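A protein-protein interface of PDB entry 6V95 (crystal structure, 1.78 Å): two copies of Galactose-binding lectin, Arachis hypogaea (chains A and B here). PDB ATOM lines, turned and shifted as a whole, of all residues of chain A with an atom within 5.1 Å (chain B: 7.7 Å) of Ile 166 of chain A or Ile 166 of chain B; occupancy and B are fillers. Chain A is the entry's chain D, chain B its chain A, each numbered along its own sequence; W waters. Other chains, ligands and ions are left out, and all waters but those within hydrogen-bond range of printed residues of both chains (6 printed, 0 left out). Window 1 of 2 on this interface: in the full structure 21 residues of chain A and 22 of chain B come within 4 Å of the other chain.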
ATOM      1  N   PHE A  65     -26.783  20.550  17.298  1.00  0.00           N
ATOM      2  CA  PHE A  65     -27.624  21.055  16.212  1.00  0.00           C
ATOM      3  C   PHE A  65     -27.174  22.418  15.738  1.00  0.00           C
ATOM      4  O   PHE A  65     -26.514  23.165  16.465  1.00  0.00           O
ATOM      5  CB  PHE A  65     -29.131  21.049  16.513  1.00  0.00           C
ATOM      6  CG  PHE A  65     -29.626  21.961  17.603  1.00  0.00           C
ATOM      7  CD1 PHE A  65     -29.805  23.321  17.368  1.00  0.00           C
ATOM      8  CD2 PHE A  65     -30.020  21.447  18.839  1.00  0.00           C
ATOM      9  CE1 PHE A  65     -30.330  24.152  18.353  1.00  0.00           C
ATOM     10  CE2 PHE A  65     -30.527  22.281  19.824  1.00  0.00           C
ATOM     11  CZ  PHE A  65     -30.673  23.628  19.583  1.00  0.00           C
ATOM     12  N   LEU A  66     -27.524  22.709  14.486  1.00  0.00           N
ATOM     13  CA  LEU A  66     -27.283  23.969  13.797  1.00  0.00           C
ATOM     14  C   LEU A  66     -28.580  24.375  13.165  1.00  0.00           C
ATOM     15  O   LEU A  66     -29.152  23.607  12.384  1.00  0.00           O
ATOM     16  CB  LEU A  66     -26.175  23.852  12.736  1.00  0.00           C
ATOM     17  CG  LEU A  66     -26.034  25.033  11.763  1.00  0.00           C
ATOM     18  CD1 LEU A  66     -25.553  26.308  12.472  1.00  0.00           C
ATOM     19  CD2 LEU A  66     -25.097  24.662  10.590  1.00  0.00           C
ATOM     20  N   THR A 164     -28.726  32.633  13.653  1.00  0.00           N
ATOM     21  CA  THR A 164     -28.009  31.377  13.564  1.00  0.00           C
ATOM     22  C   THR A 164     -27.823  30.884  15.004  1.00  0.00           C
ATOM     23  O   THR A 164     -27.416  31.662  15.880  1.00  0.00           O
ATOM     24  CB  THR A 164     -26.703  31.508  12.812  1.00  0.00           C
ATOM     25  OG1 THR A 164     -26.989  31.791  11.439  1.00  0.00           O
ATOM     26  CG2 THR A 164     -25.872  30.211  12.894  1.00  0.00           C
ATOM     27  N   VAL A 165     -28.159  29.608  15.245  1.00  0.00           N
ATOM     28  CA  VAL A 165     -28.045  28.998  16.570  1.00  0.00           C
ATOM     29  C   VAL A 165     -27.210  27.718  16.476  1.00  0.00           C
ATOM     30  O   VAL A 165     -27.472  26.874  15.615  1.00  0.00           O
ATOM     31  CB  VAL A 165     -29.428  28.720  17.228  1.00  0.00           C
ATOM     32  CG1 VAL A 165     -29.254  28.075  18.602  1.00  0.00           C
ATOM     33  CG2 VAL A 165     -30.283  29.982  17.340  1.00  0.00           C
ATOM     34  N   ILE A 166     -26.224  27.571  17.373  1.00  0.00           N
ATOM     35  CA  ILE A 166     -25.415  26.356  17.464  1.00  0.00           C
ATOM     36  C   ILE A 166     -25.599  25.775  18.866  1.00  0.00           C
ATOM     37  O   ILE A 166     -25.337  26.464  19.864  1.00  0.00           O
ATOM     38  CB  ILE A 166     -23.896  26.554  17.163  1.00  0.00           C
ATOM     39  CG1 ILE A 166     -23.629  27.171  15.769  1.00  0.00           C
ATOM     40  CG2 ILE A 166     -23.100  25.231  17.359  1.00  0.00           C
ATOM     41  CD1 ILE A 166     -22.179  27.618  15.578  1.00  0.00           C
ATOM     42  N   TYR A 167     -25.945  24.491  18.939  1.00  0.00           N
ATOM     43  CA  TYR A 167     -25.924  23.798  20.227  1.00  0.00           C
ATOM     44  C   TYR A 167     -24.803  22.752  20.161  1.00  0.00           C
ATOM     45  O   TYR A 167     -24.874  21.819  19.356  1.00  0.00           O
ATOM     46  CB  TYR A 167     -27.259  23.183  20.637  1.00  0.00           C
ATOM     47  CG  TYR A 167     -27.186  22.536  21.999  1.00  0.00           C
ATOM     48  CD1 TYR A 167     -27.058  23.307  23.156  1.00  0.00           C
ATOM     49  CD2 TYR A 167     -27.110  21.147  22.130  1.00  0.00           C
ATOM     50  CE1 TYR A 167     -26.933  22.712  24.414  1.00  0.00           C
ATOM     51  CE2 TYR A 167     -26.980  20.544  23.382  1.00  0.00           C
ATOM     52  CZ  TYR A 167     -26.910  21.332  24.520  1.00  0.00           C
ATOM     53  OH  TYR A 167     -26.826  20.760  25.763  1.00  0.00           O
ATOM     54  N   ASP A 168     -23.765  22.930  20.991  1.00  0.00           N
ATOM     55  CA  ASP A 168     -22.640  21.998  21.069  1.00  0.00           C
ATOM     56  C   ASP A 168     -22.890  21.033  22.248  1.00  0.00           C
ATOM     57  O   ASP A 168     -22.796  21.459  23.409  1.00  0.00           O
ATOM     58  CB  ASP A 168     -21.325  22.753  21.243  1.00  0.00           C
ATOM     59  CG  ASP A 168     -20.159  21.805  21.431  1.00  0.00           C
ATOM     60  OD1 ASP A 168     -19.832  21.071  20.475  1.00  0.00           O
ATOM     61  OD2 ASP A 168     -19.610  21.769  22.537  1.00  0.00           O
ATOM     62  N   THR A 173     -23.268  23.972  25.364  1.00  0.00           N
ATOM     63  CA  THR A 173     -23.396  25.404  25.074  1.00  0.00           C
ATOM     64  C   THR A 173     -24.361  25.684  23.947  1.00  0.00           C
ATOM     65  O   THR A 173     -24.187  25.161  22.844  1.00  0.00           O
ATOM     66  CB  THR A 173     -22.033  26.018  24.722  1.00  0.00           C
ATOM     67  OG1 THR A 173     -21.163  25.825  25.846  1.00  0.00           O
ATOM     68  CG2 THR A 173     -22.132  27.517  24.363  1.00  0.00           C
ATOM     69  N   LEU A 174     -25.325  26.571  24.224  1.00  0.00           N
ATOM     70  CA  LEU A 174     -26.289  27.125  23.276  1.00  0.00           C
ATOM     71  C   LEU A 174     -25.772  28.525  22.867  1.00  0.00           C
ATOM     72  O   LEU A 174     -25.703  29.423  23.717  1.00  0.00           O
ATOM     73  CB  LEU A 174     -27.703  27.206  23.894  1.00  0.00           C
ATOM     74  CG  LEU A 174     -28.858  27.587  22.925  1.00  0.00           C
ATOM     75  CD1 LEU A 174     -29.132  26.491  21.909  1.00  0.00           C
ATOM     76  CD2 LEU A 174     -30.128  27.859  23.682  1.00  0.00           C
ATOM     77  N   SER A 175     -25.284  28.661  21.623  1.00  0.00           N
ATOM     78  CA  SER A 175     -24.777  29.946  21.102  1.00  0.00           C
ATOM     79  C   SER A 175     -25.743  30.504  20.056  1.00  0.00           C
ATOM     80  O   SER A 175     -26.202  29.766  19.172  1.00  0.00           O
ATOM     81  CB  SER A 175     -23.390  29.768  20.496  1.00  0.00           C
ATOM     82  OG  SER A 175     -22.452  29.318  21.460  1.00  0.00           O
ATOM     83  N   VAL A 176     -26.009  31.824  20.122  1.00  0.00           N
ATOM     84  CA  VAL A 176     -26.957  32.541  19.253  1.00  0.00           C
ATOM     85  C   VAL A 176     -26.281  33.779  18.641  1.00  0.00           C
ATOM     86  O   VAL A 176     -25.674  34.575  19.378  1.00  0.00           O
ATOM     87  CB  VAL A 176     -28.205  32.974  20.087  1.00  0.00           C
ATOM     88  CG1 VAL A 176     -29.248  33.706  19.242  1.00  0.00           C
ATOM     89  CG2 VAL A 176     -28.843  31.780  20.821  1.00  0.00           C
ATOM     90  N   ALA A 177     -26.400  33.939  17.312  1.00  0.00           N
ATOM     91  CA  ALA A 177     -25.928  35.129  16.576  1.00  0.00           C
ATOM     92  C   ALA A 177     -27.110  35.701  15.802  1.00  0.00           C
ATOM     93  O   ALA A 177     -27.772  34.975  15.022  1.00  0.00           O
ATOM     94  CB  ALA A 177     -24.758  34.797  15.652  1.00  0.00           C
ATOM     95  N   THR A 187     -24.811  38.748  19.900  1.00  0.00           N
ATOM     96  CA  THR A 187     -24.606  37.350  20.301  1.00  0.00           C
ATOM     97  C   THR A 187     -24.975  37.175  21.749  1.00  0.00           C
ATOM     98  O   THR A 187     -24.899  38.127  22.552  1.00  0.00           O
ATOM     99  CB  THR A 187     -23.178  36.827  20.054  1.00  0.00           C
ATOM    100  OG1 THR A 187     -22.251  37.460  20.935  1.00  0.00           O
ATOM    101  CG2 THR A 187     -22.732  36.912  18.605  1.00  0.00           C
ATOM    102  N   SER B  64     -17.858  40.502  19.235  1.00  0.00           N
ATOM    103  CA  SER B  64     -18.448  39.205  18.910  1.00  0.00           C
ATOM    104  C   SER B  64     -18.337  39.088  17.422  1.00  0.00           C
ATOM    105  O   SER B  64     -18.237  40.131  16.751  1.00  0.00           O
ATOM    106  CB  SER B  64     -19.910  39.114  19.355  1.00  0.00           C
ATOM    107  OG  SER B  64     -19.992  38.888  20.752  1.00  0.00           O
ATOM    108  N   PHE B  65     -18.355  37.870  16.873  1.00  0.00           N
ATOM    109  CA  PHE B  65     -18.353  37.700  15.432  1.00  0.00           C
ATOM    110  C   PHE B  65     -19.096  36.444  14.998  1.00  0.00           C
ATOM    111  O   PHE B  65     -19.253  35.473  15.758  1.00  0.00           O
ATOM    112  CB  PHE B  65     -16.948  37.745  14.804  1.00  0.00           C
ATOM    113  CG  PHE B  65     -15.981  36.641  15.161  1.00  0.00           C
ATOM    114  CD1 PHE B  65     -16.071  35.390  14.557  1.00  0.00           C
ATOM    115  CD2 PHE B  65     -14.919  36.880  16.018  1.00  0.00           C
ATOM    116  CE1 PHE B  65     -15.146  34.393  14.837  1.00  0.00           C
ATOM    117  CE2 PHE B  65     -13.992  35.873  16.304  1.00  0.00           C
ATOM    118  CZ  PHE B  65     -14.120  34.639  15.733  1.00  0.00           C
ATOM    119  N   LEU B  66     -19.589  36.509  13.760  1.00  0.00           N
ATOM    120  CA  LEU B  66     -20.268  35.426  13.055  1.00  0.00           C
ATOM    121  C   LEU B  66     -19.576  35.283  11.715  1.00  0.00           C
ATOM    122  O   LEU B  66     -19.471  36.262  10.964  1.00  0.00           O
ATOM    123  CB  LEU B  66     -21.766  35.700  12.879  1.00  0.00           C
ATOM    124  CG  LEU B  66     -22.499  34.790  11.876  1.00  0.00           C
ATOM    125  CD1 LEU B  66     -22.598  33.308  12.433  1.00  0.00           C
ATOM    126  CD2 LEU B  66     -23.832  35.345  11.521  1.00  0.00           C
ATOM    127  N   THR B  67     -19.118  34.087  11.405  1.00  0.00           N
ATOM    128  CA  THR B  67     -18.440  33.889  10.119  1.00  0.00           C
ATOM    129  C   THR B  67     -18.811  32.532   9.548  1.00  0.00           C
ATOM    130  O   THR B  67     -18.963  31.553  10.276  1.00  0.00           O
ATOM    131  CB  THR B  67     -16.901  34.114  10.223  1.00  0.00           C
ATOM    132  OG1 THR B  67     -16.312  34.059   8.916  1.00  0.00           O
ATOM    133  CG2 THR B  67     -16.188  33.123  11.168  1.00  0.00           C
ATOM    134  N   SER B  68     -19.006  32.494   8.242  1.00  0.00           N
ATOM    135  CA  SER B  68     -19.277  31.257   7.531  1.00  0.00           C
ATOM    136  C   SER B  68     -18.347  31.143   6.329  1.00  0.00           C
ATOM    137  O   SER B  68     -17.986  32.151   5.723  1.00  0.00           O
ATOM    138  CB  SER B  68     -20.734  31.185   7.097  1.00  0.00           C
ATOM    139  OG  SER B  68     -21.595  31.149   8.224  1.00  0.00           O
ATOM    140  N   VAL B 163     -18.905  25.629   7.011  1.00  0.00           N
ATOM    141  CA  VAL B 163     -18.558  25.899   8.395  1.00  0.00           C
ATOM    142  C   VAL B 163     -19.227  27.207   8.848  1.00  0.00           C
ATOM    143  O   VAL B 163     -19.228  28.196   8.123  1.00  0.00           O
ATOM    144  CB  VAL B 163     -17.021  25.925   8.650  1.00  0.00           C
ATOM    145  CG1 VAL B 163     -16.714  26.063  10.148  1.00  0.00           C
ATOM    146  CG2 VAL B 163     -16.334  24.677   8.077  1.00  0.00           C
ATOM    147  N   THR B 164     -19.750  27.198  10.062  1.00  0.00           N
ATOM    148  CA  THR B 164     -20.297  28.368  10.706  1.00  0.00           C
ATOM    149  C   THR B 164     -19.595  28.475  12.049  1.00  0.00           C
ATOM    150  O   THR B 164     -19.487  27.490  12.780  1.00  0.00           O
ATOM    151  CB  THR B 164     -21.818  28.320  10.813  1.00  0.00           C
ATOM    152  OG1 THR B 164     -22.365  28.430   9.505  1.00  0.00           O
ATOM    153  CG2 THR B 164     -22.365  29.481  11.646  1.00  0.00           C
ATOM    154  N   VAL B 165     -19.113  29.668  12.361  1.00  0.00           N
ATOM    155  CA  VAL B 165     -18.416  29.936  13.615  1.00  0.00           C
ATOM    156  C   VAL B 165     -19.069  31.143  14.310  1.00  0.00           C
ATOM    157  O   VAL B 165     -19.288  32.187  13.694  1.00  0.00           O
ATOM    158  CB  VAL B 165     -16.890  30.157  13.408  1.00  0.00           C
ATOM    159  CG1 VAL B 165     -16.208  30.473  14.736  1.00  0.00           C
ATOM    160  CG2 VAL B 165     -16.223  28.958  12.718  1.00  0.00           C
ATOM    161  N   ILE B 166     -19.347  30.988  15.619  1.00  0.00           N
ATOM    162  CA  ILE B 166     -19.864  32.074  16.441  1.00  0.00           C
ATOM    163  C   ILE B 166     -18.879  32.327  17.569  1.00  0.00           C
ATOM    164  O   ILE B 166     -18.577  31.401  18.334  1.00  0.00           O
ATOM    165  CB  ILE B 166     -21.289  31.810  17.020  1.00  0.00           C
ATOM    166  CG1 ILE B 166     -22.350  31.565  15.921  1.00  0.00           C
ATOM    167  CG2 ILE B 166     -21.724  32.973  17.967  1.00  0.00           C
ATOM    168  CD1 ILE B 166     -23.661  30.954  16.498  1.00  0.00           C
ATOM    169  N   TYR B 167     -18.416  33.587  17.707  1.00  0.00           N
ATOM    170  CA  TYR B 167     -17.641  33.941  18.896  1.00  0.00           C
ATOM    171  C   TYR B 167     -18.490  34.896  19.725  1.00  0.00           C
ATOM    172  O   TYR B 167     -18.843  35.988  19.262  1.00  0.00           O
ATOM    173  CB  TYR B 167     -16.264  34.533  18.581  1.00  0.00           C
ATOM    174  CG  TYR B 167     -15.477  34.844  19.842  1.00  0.00           C
ATOM    175  CD1 TYR B 167     -14.953  33.816  20.628  1.00  0.00           C
ATOM    176  CD2 TYR B 167     -15.342  36.157  20.298  1.00  0.00           C
ATOM    177  CE1 TYR B 167     -14.287  34.087  21.824  1.00  0.00           C
ATOM    178  CE2 TYR B 167     -14.666  36.443  21.490  1.00  0.00           C
ATOM    179  CZ  TYR B 167     -14.131  35.405  22.241  1.00  0.00           C
ATOM    180  OH  TYR B 167     -13.432  35.685  23.395  1.00  0.00           O
ATOM    181  N   ASP B 168     -18.866  34.463  20.923  1.00  0.00           N
ATOM    182  CA  ASP B 168     -19.659  35.281  21.852  1.00  0.00           C
ATOM    183  C   ASP B 168     -18.707  35.947  22.844  1.00  0.00           C
ATOM    184  O   ASP B 168     -18.165  35.255  23.706  1.00  0.00           O
ATOM    185  CB  ASP B 168     -20.704  34.418  22.584  1.00  0.00           C
ATOM    186  CG  ASP B 168     -21.476  35.216  23.619  1.00  0.00           C
ATOM    187  OD1 ASP B 168     -22.219  36.147  23.227  1.00  0.00           O
ATOM    188  OD2 ASP B 168     -21.280  34.970  24.811  1.00  0.00           O
ATOM    189  N   SER B 169     -18.494  37.276  22.733  1.00  0.00           N
ATOM    190  CA  SER B 169     -17.511  37.969  23.575  1.00  0.00           C
ATOM    191  C   SER B 169     -17.780  37.871  25.093  1.00  0.00           C
ATOM    192  O   SER B 169     -16.817  37.666  25.831  1.00  0.00           O
ATOM    193  CB  SER B 169     -17.368  39.431  23.170  1.00  0.00           C
ATOM    194  OG  SER B 169     -18.508  40.204  23.499  1.00  0.00           O
ATOM    195  N   LYS B 172     -16.929  34.426  26.118  1.00  0.00           N
ATOM    196  CA  LYS B 172     -15.642  34.135  25.477  1.00  0.00           C
ATOM    197  C   LYS B 172     -15.704  32.738  24.787  1.00  0.00           C
ATOM    198  O   LYS B 172     -14.688  32.055  24.658  1.00  0.00           O
ATOM    199  CB  LYS B 172     -14.466  34.226  26.481  1.00  0.00           C
ATOM    200  CG  LYS B 172     -14.309  35.622  27.112  1.00  0.00           C
ATOM    201  CD  LYS B 172     -13.305  35.627  28.264  1.00  0.00           C
ATOM    202  CE  LYS B 172     -13.120  37.017  28.850  1.00  0.00           C
ATOM    203  NZ  LYS B 172     -14.323  37.493  29.591  1.00  0.00           N
ATOM    204  N   THR B 173     -16.902  32.312  24.366  1.00  0.00           N
ATOM    205  CA  THR B 173     -17.071  31.008  23.725  1.00  0.00           C
ATOM    206  C   THR B 173     -16.917  31.096  22.221  1.00  0.00           C
ATOM    207  O   THR B 173     -17.600  31.888  21.576  1.00  0.00           O
ATOM    208  CB  THR B 173     -18.465  30.391  24.064  1.00  0.00           C
ATOM    209  OG1 THR B 173     -18.557  30.239  25.489  1.00  0.00           O
ATOM    210  CG2 THR B 173     -18.677  29.037  23.386  1.00  0.00           C
ATOM    211  N   LEU B 174     -16.029  30.246  21.680  1.00  0.00           N
ATOM    212  CA  LEU B 174     -15.829  30.014  20.250  1.00  0.00           C
ATOM    213  C   LEU B 174     -16.569  28.725  19.891  1.00  0.00           C
ATOM    214  O   LEU B 174     -16.147  27.643  20.323  1.00  0.00           O
ATOM    215  CB  LEU B 174     -14.327  29.896  19.912  1.00  0.00           C
ATOM    216  CG  LEU B 174     -13.976  29.828  18.426  1.00  0.00           C
ATOM    217  CD1 LEU B 174     -14.224  31.159  17.714  1.00  0.00           C
ATOM    218  CD2 LEU B 174     -12.523  29.433  18.231  1.00  0.00           C
ATOM    219  N   SER B 175     -17.715  28.847  19.210  1.00  0.00           N
ATOM    220  CA  SER B 175     -18.543  27.693  18.795  1.00  0.00           C
ATOM    221  C   SER B 175     -18.422  27.478  17.292  1.00  0.00           C
ATOM    222  O   SER B 175     -18.499  28.438  16.528  1.00  0.00           O
ATOM    223  CB  SER B 175     -20.010  27.888  19.185  1.00  0.00           C
ATOM    224  OG  SER B 175     -20.677  26.653  19.015  1.00  0.00           O
ATOM    225  N   VAL B 176     -18.248  26.213  16.885  1.00  0.00           N
ATOM    226  CA  VAL B 176     -18.022  25.778  15.493  1.00  0.00           C
ATOM    227  C   VAL B 176     -19.021  24.686  15.103  1.00  0.00           C
ATOM    228  O   VAL B 176     -19.160  23.699  15.840  1.00  0.00           O
ATOM    229  CB  VAL B 176     -16.557  25.259  15.320  1.00  0.00           C
ATOM    230  CG1 VAL B 176     -16.271  24.813  13.886  1.00  0.00           C
ATOM    231  CG2 VAL B 176     -15.534  26.282  15.778  1.00  0.00           C
ATOM    232  N   ALA B 177     -19.681  24.851  13.933  1.00  0.00           N
ATOM    233  CA  ALA B 177     -20.579  23.847  13.352  1.00  0.00           C
ATOM    234  C   ALA B 177     -20.109  23.569  11.939  1.00  0.00           C
ATOM    235  O   ALA B 177     -20.007  24.503  11.134  1.00  0.00           O
ATOM    236  CB  ALA B 177     -22.035  24.307  13.373  1.00  0.00           C
ATOM    237  N   VAL B 178     -19.795  22.297  11.662  1.00  0.00           N
ATOM    238  CA  VAL B 178     -19.258  21.807  10.376  1.00  0.00           C
ATOM    239  C   VAL B 178     -20.294  20.905   9.718  1.00  0.00           C
ATOM    240  O   VAL B 178     -20.662  19.876  10.303  1.00  0.00           O
ATOM    241  CB  VAL B 178     -17.915  21.064  10.580  1.00  0.00           C
ATOM    242  CG1 VAL B 178     -17.271  20.700   9.239  1.00  0.00           C
ATOM    243  CG2 VAL B 178     -16.954  21.873  11.441  1.00  0.00           C
ATOM    244  N   ILE B 185     -23.876  16.903  10.904  1.00  0.00           N
ATOM    245  CA  ILE B 185     -23.185  18.048  11.471  1.00  0.00           C
ATOM    246  C   ILE B 185     -22.212  17.583  12.534  1.00  0.00           C
ATOM    247  O   ILE B 185     -22.472  16.611  13.240  1.00  0.00           O
ATOM    248  CB  ILE B 185     -24.089  19.210  12.000  1.00  0.00           C
ATOM    249  CG1 ILE B 185     -25.226  18.720  12.885  1.00  0.00           C
ATOM    250  CG2 ILE B 185     -24.574  20.099  10.873  1.00  0.00           C
ATOM    251  CD1 ILE B 185     -25.027  19.157  14.245  1.00  0.00           C
ATOM    252  N   THR B 186     -21.072  18.273  12.623  1.00  0.00           N
ATOM    253  CA  THR B 186     -20.035  18.083  13.638  1.00  0.00           C
ATOM    254  C   THR B 186     -19.909  19.421  14.374  1.00  0.00           C
ATOM    255  O   THR B 186     -19.824  20.457  13.717  1.00  0.00           O
ATOM    256  CB  THR B 186     -18.704  17.633  12.981  1.00  0.00           C
ATOM    257  OG1 THR B 186     -18.943  16.474  12.189  1.00  0.00           O
ATOM    258  CG2 THR B 186     -17.603  17.347  13.994  1.00  0.00           C
ATOM    259  N   THR B 187     -19.881  19.410  15.709  1.00  0.00           N
ATOM    260  CA  THR B 187     -19.682  20.656  16.453  1.00  0.00           C
ATOM    261  C   THR B 187     -18.533  20.541  17.428  1.00  0.00           C
ATOM    262  O   THR B 187     -18.214  19.452  17.913  1.00  0.00           O
ATOM    263  CB  THR B 187     -20.945  21.145  17.205  1.00  0.00           C
ATOM    264  OG1 THR B 187     -21.236  20.265  18.299  1.00  0.00           O
ATOM    265  CG2 THR B 187     -22.157  21.365  16.293  1.00  0.00           C
ATOM    266  N   ILE B 188     -17.950  21.688  17.763  1.00  0.00           N
ATOM    267  CA  ILE B 188     -16.891  21.812  18.776  1.00  0.00           C
ATOM    268  C   ILE B 188     -16.962  23.251  19.308  1.00  0.00           C
ATOM    269  O   ILE B 188     -17.186  24.189  18.544  1.00  0.00           O
ATOM    270  CB  ILE B 188     -15.466  21.410  18.264  1.00  0.00           C
ATOM    271  CG1 ILE B 188     -14.457  21.345  19.444  1.00  0.00           C
ATOM    272  CG2 ILE B 188     -14.962  22.294  17.086  1.00  0.00           C
ATOM    273  CD1 ILE B 188     -13.057  20.786  19.104  1.00  0.00           C
ATOM    274  N   ALA B 189     -16.817  23.407  20.612  1.00  0.00           N
ATOM    275  CA  ALA B 189     -16.859  24.711  21.265  1.00  0.00           C
ATOM    276  C   ALA B 189     -15.814  24.755  22.369  1.00  0.00           C
ATOM    277  O   ALA B 189     -15.505  23.734  22.984  1.00  0.00           O
ATOM    278  CB  ALA B 189     -18.263  25.020  21.799  1.00  0.00           C
ATOM    279  N   GLN B 190     -15.243  25.932  22.584  1.00  0.00           N
ATOM    280  CA  GLN B 190     -14.184  26.133  23.591  1.00  0.00           C
ATOM    281  C   GLN B 190     -14.181  27.574  24.048  1.00  0.00           C
ATOM    282  O   GLN B 190     -14.253  28.482  23.218  1.00  0.00           O
ATOM    283  CB  GLN B 190     -12.804  25.766  22.975  1.00  0.00           C
ATOM    284  CG  GLN B 190     -11.559  25.986  23.869  1.00  0.00           C
ATOM    285  CD  GLN B 190     -11.645  25.139  25.135  1.00  0.00           C
ATOM    286  OE1 GLN B 190     -11.851  23.922  25.084  1.00  0.00           O
ATOM    287  NE2 GLN B 190     -11.555  25.777  26.301  1.00  0.00           N
HETATM  288  O   HOH W   1     -19.306  27.608  27.156  1.00  0.00           O
HETATM  289  O   HOH W   2     -21.589  38.793  24.057  1.00  0.00           O
HETATM  290  O   HOH W   3     -20.327  31.020  20.942  1.00  0.00           O
HETATM  291  O   HOH W   4     -20.130  18.342  20.914  1.00  0.00           O
HETATM  292  O   HOH W   5     -16.943  20.773  22.229  1.00  0.00           O
HETATM  293  O   HOH W   6     -22.345  26.576  21.145  1.00  0.00           O
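OG1 of Thr 187 of chain A is in hydrogen-bond range of OG of Ser 64 of chain B (2.7 Å).
The side-chain carboxylate (OD1) of Asp 168 of chain B sits at hydrogen-bond distance from the side-chain hydroxyl (OG1) of Thr 187 of chain A (2.6 Å).
The side-chain carboxylate (OD1) of Asp 168 of chain A is in hydrogen-bond range of the side-chain hydroxyl (OG1) of Thr 187 of chain B, 2.7 Å away.
The side-chain carboxylate (OD1) of Asp 168 of chain A sits at hydrogen-bond distance from the backbone NH (N) of Ile 188 of chain B (3.4 Å).
OG of Ser 64 of chain B lies close to O of Tyr 167 of chain B (3.5 Å).
The side-chain hydroxyl of Ser 64 of chain B lies within hydrogen-bond range of the backbone NH of Ser 169 of chain B, at 3.0 Å.
The backbone carbonyl oxygen (O) of Thr 164 of chain B sits at hydrogen-bond distance from the backbone NH (N) of Ala 177 of chain B (2.9 Å).
The backbone NH (N) of Asp 168 of chain B lies within hydrogen-bond range of the backbone carbonyl oxygen (O) of Thr 173 of chain B, at 2.9 Å.
O of Ile 166 of chain A lies within hydrogen-bond range of N of Ser 175 of chain A (2.8 Å).
Among the printed residues, pairs that only touch across the chains: Ile 166 of chain A with Ser 175 of chain B (3.3 Å), Asp 168 of chain A with Ala 189 of chain B (3.6 Å), Ser 175 of chain A with Ser 175 of chain B (3.6 Å), Ile 166 of chain A with Ile 166 of chain B (3.8 Å), Phe 65 of chain A with Ile 185 of chain B (3.8 Å), Thr 164 of chain A with Thr 164 of chain B (3.8 Å), Thr 164 of chain A with Ile 166 of chain B (3.9 Å), Ser 175 of chain A with Ile 166 of chain B (3.9 Å), Ile 166 of chain A with Thr 164 of chain B (3.9 Å), Thr 173 of chain A with Thr 173 of chain B (3.9 Å) and Ile 166 of chain A with Ala 177 of chain B (3.98 Å).
Of the printed residues of chain B, Ile 166 of chain A touches Thr 164 (3.9 Å), Ile 166 (3.8 Å), Ser 175 (3.3 Å) and Ala 177 (3.98 Å).
Of the printed residues of chain B, Thr 173 of chain A touches Thr 173.
Phe 65 of chain B touches none of the printed residues of chain A.
Of the printed residues of chain A, Ile 166 of chain B touches Thr 164 (3.9 Å), Ile 166 (3.8 Å) and Ser 175 (3.9 Å).
Printed residues of chain A within 4 Å of Ala 177 of chain B: Ile 166.
Of the printed residues of chain A, Thr 187 of chain B touches Asp 168 (2.7 Å).
The nearest printed residue of chain B that does not touch Ile 166 of chain A is Thr 187 of chain B (4.1 Å).
The nearest printed residue of chain A that does not touch Ile 188 of chain B is Ile 166 of chain A (6.1 Å).
Of the 25 printed residues of chain B, 11 touch a printed residue of chain A.
Hydrophobic or aromatic side chains of chain B that line the printed part of chain A: Ile 166, Ala 177, Ile 185 and Ala 189.
Hydrophobic or aromatic side chains of chain A that line the printed part of chain B: Ile 166.
Among the printed residues, 15 pairs touch across the chains.
Among the printed residues, no Asp or Glu carboxylate lies within 4 Å of a Lys or Arg side-chain nitrogen of the other chain.
Thr 164 of chain A touches Ile 166 of chain B, and with the chains exchanged Ile 166 of chain A touches Thr 164 of chain B.
Ile 166 of chain A touches Ala 177 of chain B, but with the chains exchanged Ala 177 of chain A does not touch Ile 166 of chain B (4.04 Å).
Asp 168 of chain A touches Thr 187 of chain B, and with the chains exchanged Thr 187 of chain A touches Asp 168 of chain B.
Ser 175 of chain A touches its own counterpart, Ser 175 of chain B.
Water W6 lies within hydrogen-bond range of OG of Ser 175 of chain B, OG of Ser 175 of chain A, O of Thr 173 of chain A and O of Ile 166 of chain A.
Water W3 lies within hydrogen-bond range of the side-chain hydroxyl (OG) of Ser 175 of chain A (2.8 Å), the backbone carbonyl oxygen (O) of Thr 173 of chain B (2.9 Å) and the backbone carbonyl oxygen (O) of Ile 166 of chain B (3.2 Å).
Water W2 lies within hydrogen-bond range of OD1 of Asp 168 of chain B (2.8 Å), OG of Ser 169 of chain B (3.4 Å) and OG1 of Thr 187 of chain A (3.5 Å).
Water W5 lies within hydrogen-bond range of the side-chain carboxylate (OD2) of Asp 168 of chain A (2.9 Å) and the backbone NH (N) of Ala 189 of chain B (3.1 Å).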
